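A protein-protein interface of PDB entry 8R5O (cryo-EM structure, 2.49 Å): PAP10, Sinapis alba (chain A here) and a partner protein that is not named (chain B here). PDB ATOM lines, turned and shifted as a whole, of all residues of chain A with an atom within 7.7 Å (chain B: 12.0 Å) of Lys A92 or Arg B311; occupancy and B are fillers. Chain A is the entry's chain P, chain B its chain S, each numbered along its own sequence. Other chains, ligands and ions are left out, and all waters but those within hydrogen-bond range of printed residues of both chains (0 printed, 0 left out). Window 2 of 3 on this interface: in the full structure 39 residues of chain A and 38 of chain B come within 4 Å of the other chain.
Hydrophobic or aromatic side chains of chain A that line the printed part of chain B: Val A91. Among the printed residues, 7 pairs touch across the chains.
Among the printed residues, pairs that only touch across the chains: Gln A88 with Gly B312, Gln A88 with Arg B313, Val A91 with Lys B310, Lys A92 with Lys B310, Lys A92 with Arg B311, Lys A92 with Gly B312 and Gly A93 with Lys B310.
No residue of chain B comes within 4 Å of Asp A89. Printed residues of chain B within 4 Å of Val A91: Lys B310. Lys A92 touches three residues of chain B. Of chain B, only Lys B310 comes within 4 Å of Gly A93. No residue of chain B comes within 4 Å of Glu A94. Ile B308 touches none of the printed residues of chain A. Printed residues of chain A within 4 Å of Lys B310: Val A91 (3.5 Å), Lys A92 (3.5 Å) and Gly A93 (3.98 Å). Arg B311 touches just one residue of chain A: Lys A92 (3.8 Å). Gly B312 touches just these residues of chain A: Gln A88 (3.5 Å) and Lys A92 (3.6 Å). Printed residues of chain A within 4 Å of Arg B313: Gln A88 (3.9 Å).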
ATOM      1  N   GLU A  86     -19.730   7.965  30.341  1.00  0.00           N
ATOM      2  CA  GLU A  86     -20.882   7.091  30.149  1.00  0.00           C
ATOM      3  C   GLU A  86     -21.744   7.568  28.989  1.00  0.00           C
ATOM      4  O   GLU A  86     -22.258   6.755  28.211  1.00  0.00           O
ATOM      5  CB  GLU A  86     -21.703   7.016  31.436  1.00  0.00           C
ATOM      6  CG  GLU A  86     -21.018   6.259  32.560  1.00  0.00           C
ATOM      7  CD  GLU A  86     -21.927   6.030  33.750  1.00  0.00           C
ATOM      8  OE1 GLU A  86     -22.317   7.022  34.402  1.00  0.00           O
ATOM      9  OE2 GLU A  86     -22.256   4.859  34.030  1.00  0.00           O
ATOM     10  N   LEU A  87     -21.919   8.884  28.859  1.00  0.00           N
ATOM     11  CA  LEU A  87     -22.716   9.420  27.761  1.00  0.00           C
ATOM     12  C   LEU A  87     -22.019   9.237  26.421  1.00  0.00           C
ATOM     13  O   LEU A  87     -22.684   8.999  25.407  1.00  0.00           O
ATOM     14  CB  LEU A  87     -23.022  10.897  28.002  1.00  0.00           C
ATOM     15  CG  LEU A  87     -24.053  11.527  27.066  1.00  0.00           C
ATOM     16  CD1 LEU A  87     -25.336  10.713  27.070  1.00  0.00           C
ATOM     17  CD2 LEU A  87     -24.328  12.960  27.473  1.00  0.00           C
ATOM     18  N   GLN A  88     -20.690   9.355  26.391  1.00  0.00           N
ATOM     19  CA  GLN A  88     -19.954   9.082  25.162  1.00  0.00           C
ATOM     20  C   GLN A  88     -20.131   7.629  24.735  1.00  0.00           C
ATOM     21  O   GLN A  88     -20.343   7.336  23.554  1.00  0.00           O
ATOM     22  CB  GLN A  88     -18.476   9.422  25.353  1.00  0.00           C
ATOM     23  CG  GLN A  88     -17.658   9.376  24.078  1.00  0.00           C
ATOM     24  CD  GLN A  88     -16.274   9.967  24.253  1.00  0.00           C
ATOM     25  OE1 GLN A  88     -15.626  10.360  23.283  1.00  0.00           O
ATOM     26  NE2 GLN A  88     -15.811  10.034  25.496  1.00  0.00           N
ATOM     27  N   ASP A  89     -20.055   6.703  25.694  1.00  0.00           N
ATOM     28  CA  ASP A  89     -20.322   5.299  25.400  1.00  0.00           C
ATOM     29  C   ASP A  89     -21.765   5.084  24.968  1.00  0.00           C
ATOM     30  O   ASP A  89     -22.061   4.134  24.234  1.00  0.00           O
ATOM     31  CB  ASP A  89     -19.997   4.439  26.621  1.00  0.00           C
ATOM     32  CG  ASP A  89     -20.450   3.000  26.461  1.00  0.00           C
ATOM     33  OD1 ASP A  89     -19.773   2.238  25.737  1.00  0.00           O
ATOM     34  OD2 ASP A  89     -21.486   2.632  27.054  1.00  0.00           O
ATOM     35  N   LEU A  90     -22.673   5.954  25.405  1.00  0.00           N
ATOM     36  CA  LEU A  90     -24.087   5.821  25.082  1.00  0.00           C
ATOM     37  C   LEU A  90     -24.451   6.482  23.759  1.00  0.00           C
ATOM     38  O   LEU A  90     -25.404   6.047  23.100  1.00  0.00           O
ATOM     39  CB  LEU A  90     -24.929   6.414  26.213  1.00  0.00           C
ATOM     40  CG  LEU A  90     -26.442   6.209  26.185  1.00  0.00           C
ATOM     41  CD1 LEU A  90     -26.780   4.730  26.154  1.00  0.00           C
ATOM     42  CD2 LEU A  90     -27.074   6.879  27.391  1.00  0.00           C
ATOM     43  N   VAL A  91     -23.717   7.514  23.352  1.00  0.00           N
ATOM     44  CA  VAL A  91     -23.979   8.183  22.080  1.00  0.00           C
ATOM     45  C   VAL A  91     -23.295   7.463  20.923  1.00  0.00           C
ATOM     46  O   VAL A  91     -23.906   7.254  19.872  1.00  0.00           O
ATOM     47  CB  VAL A  91     -23.544   9.661  22.164  1.00  0.00           C
ATOM     48  CG1 VAL A  91     -23.520  10.292  20.783  1.00  0.00           C
ATOM     49  CG2 VAL A  91     -24.479  10.437  23.085  1.00  0.00           C
ATOM     50  N   LYS A  92     -22.028   7.076  21.102  1.00  0.00           N
ATOM     51  CA  LYS A  92     -21.315   6.356  20.050  1.00  0.00           C
ATOM     52  C   LYS A  92     -21.994   5.033  19.725  1.00  0.00           C
ATOM     53  O   LYS A  92     -22.018   4.607  18.564  1.00  0.00           O
ATOM     54  CB  LYS A  92     -19.860   6.124  20.458  1.00  0.00           C
ATOM     55  CG  LYS A  92     -19.018   7.388  20.490  1.00  0.00           C
ATOM     56  CD  LYS A  92     -17.538   7.066  20.622  1.00  0.00           C
ATOM     57  CE  LYS A  92     -16.695   8.322  20.477  1.00  0.00           C
ATOM     58  NZ  LYS A  92     -15.243   8.009  20.392  1.00  0.00           N
ATOM     59  N   GLY A  93     -22.546   4.366  20.734  1.00  0.00           N
ATOM     60  CA  GLY A  93     -23.302   3.149  20.516  1.00  0.00           C
ATOM     61  C   GLY A  93     -24.581   3.384  19.741  1.00  0.00           C
ATOM     62  O   GLY A  93     -24.777   4.458  19.163  1.00  0.00           O
ATOM     63  N   GLU A  94     -25.465   2.395  19.720  1.00  0.00           N
ATOM     64  CA  GLU A  94     -26.699   2.488  18.958  1.00  0.00           C
ATOM     65  C   GLU A  94     -27.877   2.056  19.819  1.00  0.00           C
ATOM     66  O   GLU A  94     -27.727   1.317  20.796  1.00  0.00           O
ATOM     67  CB  GLU A  94     -26.631   1.646  17.680  1.00  0.00           C
ATOM     68  CG  GLU A  94     -25.693   2.219  16.631  1.00  0.00           C
ATOM     69  CD  GLU A  94     -25.340   1.218  15.552  1.00  0.00           C
ATOM     70  OE1 GLU A  94     -25.496   0.002  15.796  1.00  0.00           O
ATOM     71  OE2 GLU A  94     -24.907   1.646  14.461  1.00  0.00           O
ATOM     72  N   ARG A  95     -29.056   2.535  19.436  1.00  0.00           N
ATOM     73  CA  ARG A  95     -30.268   2.328  20.211  1.00  0.00           C
ATOM     74  C   ARG A  95     -31.453   2.374  19.257  1.00  0.00           C
ATOM     75  O   ARG A  95     -31.330   2.792  18.103  1.00  0.00           O
ATOM     76  CB  ARG A  95     -30.383   3.374  21.329  1.00  0.00           C
ATOM     77  CG  ARG A  95     -31.462   3.103  22.368  1.00  0.00           C
ATOM     78  CD  ARG A  95     -31.488   1.640  22.781  1.00  0.00           C
ATOM     79  NE  ARG A  95     -32.650   1.336  23.608  1.00  0.00           N
ATOM     80  CZ  ARG A  95     -33.166   0.124  23.764  1.00  0.00           C
ATOM     81  NH1 ARG A  95     -32.653  -0.929  23.150  1.00  0.00           N
ATOM     82  NH2 ARG A  95     -34.229  -0.032  24.547  1.00  0.00           N
ATOM     83  N   LEU A  99     -32.919   9.519  22.564  1.00  0.00           N
ATOM     84  CA  LEU A  99     -32.152   9.767  23.780  1.00  0.00           C
ATOM     85  C   LEU A  99     -32.294  11.232  24.167  1.00  0.00           C
ATOM     86  O   LEU A  99     -32.036  12.120  23.348  1.00  0.00           O
ATOM     87  CB  LEU A  99     -30.680   9.404  23.573  1.00  0.00           C
ATOM     88  CG  LEU A  99     -29.687   9.872  24.638  1.00  0.00           C
ATOM     89  CD1 LEU A  99     -29.981   9.212  25.971  1.00  0.00           C
ATOM     90  CD2 LEU A  99     -28.265   9.586  24.190  1.00  0.00           C
ATOM     91  N   LYS B 307     -25.285  19.544  14.909  1.00  0.00           N
ATOM     92  CA  LYS B 307     -24.677  18.407  14.224  1.00  0.00           C
ATOM     93  C   LYS B 307     -23.622  17.813  15.152  1.00  0.00           C
ATOM     94  O   LYS B 307     -22.471  18.257  15.164  1.00  0.00           O
ATOM     95  CB  LYS B 307     -24.070  18.822  12.887  1.00  0.00           C
ATOM     96  CG  LYS B 307     -23.551  17.655  12.054  1.00  0.00           C
ATOM     97  CD  LYS B 307     -22.040  17.715  11.876  1.00  0.00           C
ATOM     98  CE  LYS B 307     -21.628  18.896  11.012  1.00  0.00           C
ATOM     99  NZ  LYS B 307     -20.160  18.908  10.748  1.00  0.00           N
ATOM    100  N   ILE B 308     -24.006  16.787  15.904  1.00  0.00           N
ATOM    101  CA  ILE B 308     -23.119  16.208  16.905  1.00  0.00           C
ATOM    102  C   ILE B 308     -22.127  15.277  16.222  1.00  0.00           C
ATOM    103  O   ILE B 308     -22.516  14.365  15.482  1.00  0.00           O
ATOM    104  CB  ILE B 308     -23.921  15.473  17.989  1.00  0.00           C
ATOM    105  CG1 ILE B 308     -24.956  16.412  18.612  1.00  0.00           C
ATOM    106  CG2 ILE B 308     -22.992  14.935  19.063  1.00  0.00           C
ATOM    107  CD1 ILE B 308     -25.675  15.819  19.800  1.00  0.00           C
ATOM    108  N   SER B 309     -20.842  15.506  16.472  1.00  0.00           N
ATOM    109  CA  SER B 309     -19.783  14.703  15.880  1.00  0.00           C
ATOM    110  C   SER B 309     -19.604  13.409  16.663  1.00  0.00           C
ATOM    111  O   SER B 309     -19.505  13.425  17.893  1.00  0.00           O
ATOM    112  CB  SER B 309     -18.476  15.494  15.854  1.00  0.00           C
ATOM    113  OG  SER B 309     -17.419  14.724  15.314  1.00  0.00           O
ATOM    114  N   LYS B 310     -19.567  12.286  15.948  1.00  0.00           N
ATOM    115  CA  LYS B 310     -19.372  10.967  16.543  1.00  0.00           C
ATOM    116  C   LYS B 310     -18.052  10.341  16.103  1.00  0.00           C
ATOM    117  O   LYS B 310     -17.975   9.138  15.843  1.00  0.00           O
ATOM    118  CB  LYS B 310     -20.532  10.035  16.203  1.00  0.00           C
ATOM    119  CG  LYS B 310     -21.871  10.451  16.781  1.00  0.00           C
ATOM    120  CD  LYS B 310     -22.710   9.230  17.137  1.00  0.00           C
ATOM    121  CE  LYS B 310     -22.820   8.257  15.972  1.00  0.00           C
ATOM    122  NZ  LYS B 310     -23.462   6.974  16.379  1.00  0.00           N
ATOM    123  N   ARG B 311     -16.996  11.148  16.011  1.00  0.00           N
ATOM    124  CA  ARG B 311     -15.685  10.663  15.607  1.00  0.00           C
ATOM    125  C   ARG B 311     -14.693  10.668  16.762  1.00  0.00           C
ATOM    126  O   ARG B 311     -14.116   9.626  17.088  1.00  0.00           O
ATOM    127  CB  ARG B 311     -15.150  11.499  14.437  1.00  0.00           C
ATOM    128  CG  ARG B 311     -16.090  11.577  13.247  1.00  0.00           C
ATOM    129  CD  ARG B 311     -15.360  12.071  12.012  1.00  0.00           C
ATOM    130  NE  ARG B 311     -16.249  12.202  10.865  1.00  0.00           N
ATOM    131  CZ  ARG B 311     -15.841  12.420   9.622  1.00  0.00           C
ATOM    132  NH1 ARG B 311     -14.556  12.508   9.324  1.00  0.00           N
ATOM    133  NH2 ARG B 311     -16.745  12.549   8.655  1.00  0.00           N
ATOM    134  N   GLY B 312     -14.480  11.816  17.396  1.00  0.00           N
ATOM    135  CA  GLY B 312     -13.620  11.891  18.560  1.00  0.00           C
ATOM    136  C   GLY B 312     -14.397  12.273  19.802  1.00  0.00           C
ATOM    137  O   GLY B 312     -15.473  11.727  20.058  1.00  0.00           O
ATOM    138  N   ARG B 313     -13.862  13.208  20.584  1.00  0.00           N
ATOM    139  CA  ARG B 313     -14.632  13.784  21.677  1.00  0.00           C
ATOM    140  C   ARG B 313     -15.858  14.502  21.121  1.00  0.00           C
ATOM    141  O   ARG B 313     -15.825  15.079  20.032  1.00  0.00           O
ATOM    142  CB  ARG B 313     -13.767  14.747  22.490  1.00  0.00           C
ATOM    143  CG  ARG B 313     -13.270  15.946  21.706  1.00  0.00           C
ATOM    144  CD  ARG B 313     -11.882  16.368  22.155  1.00  0.00           C
ATOM    145  NE  ARG B 313     -10.919  15.283  22.010  1.00  0.00           N
ATOM    146  CZ  ARG B 313      -9.605  15.448  21.957  1.00  0.00           C
ATOM    147  NH1 ARG B 313      -9.059  16.652  22.002  1.00  0.00           N
ATOM    148  NH2 ARG B 313      -8.821  14.381  21.850  1.00  0.00           N
ATOM    149  N   LEU B 314     -16.953  14.446  21.875  1.00  0.00           N
ATOM    150  CA  LEU B 314     -18.227  14.955  21.385  1.00  0.00           C
ATOM    151  C   LEU B 314     -18.188  16.469  21.211  1.00  0.00           C
ATOM    152  O   LEU B 314     -17.751  17.200  22.106  1.00  0.00           O
ATOM    153  CB  LEU B 314     -19.354  14.561  22.337  1.00  0.00           C
ATOM    154  CG  LEU B 314     -19.760  13.086  22.334  1.00  0.00           C
ATOM    155  CD1 LEU B 314     -20.764  12.797  23.436  1.00  0.00           C
ATOM    156  CD2 LEU B 314     -20.328  12.695  20.980  1.00  0.00           C
ATOM    157  N   LYS B 315     -18.651  16.933  20.050  1.00  0.00           N
ATOM    158  CA  LYS B 315     -18.797  18.348  19.746  1.00  0.00           C
ATOM    159  C   LYS B 315     -20.180  18.560  19.144  1.00  0.00           C
ATOM    160  O   LYS B 315     -20.845  17.610  18.733  1.00  0.00           O
ATOM    161  CB  LYS B 315     -17.717  18.849  18.778  1.00  0.00           C
ATOM    162  CG  LYS B 315     -16.287  18.670  19.259  1.00  0.00           C
ATOM    163  CD  LYS B 315     -16.040  19.394  20.567  1.00  0.00           C
ATOM    164  CE  LYS B 315     -14.601  19.872  20.666  1.00  0.00           C
ATOM    165  NZ  LYS B 315     -13.629  18.825  20.241  1.00  0.00           N
ATOM    166  N   SER B 316     -20.609  19.821  19.089  1.00  0.00           N
ATOM    167  CA  SER B 316     -21.981  20.136  18.709  1.00  0.00           C
ATOM    168  C   SER B 316     -22.092  20.926  17.414  1.00  0.00           C
ATOM    169  O   SER B 316     -22.814  20.498  16.507  1.00  0.00           O
ATOM    170  CB  SER B 316     -22.666  20.893  19.851  1.00  0.00           C
ATOM    171  OG  SER B 316     -21.746  21.780  20.452  1.00  0.00           O
ATOM    172  N   THR B 317     -21.427  22.076  17.303  1.00  0.00           N
ATOM    173  CA  THR B 317     -21.329  22.822  16.043  1.00  0.00           C
ATOM    174  C   THR B 317     -22.710  23.087  15.429  1.00  0.00           C
ATOM    175  O   THR B 317     -23.091  22.511  14.411  1.00  0.00           O
ATOM    176  CB  THR B 317     -20.420  22.098  15.043  1.00  0.00           C
ATOM    177  OG1 THR B 317     -21.058  20.896  14.593  1.00  0.00           O
ATOM    178  CG2 THR B 317     -19.089  21.752  15.690  1.00  0.00           C
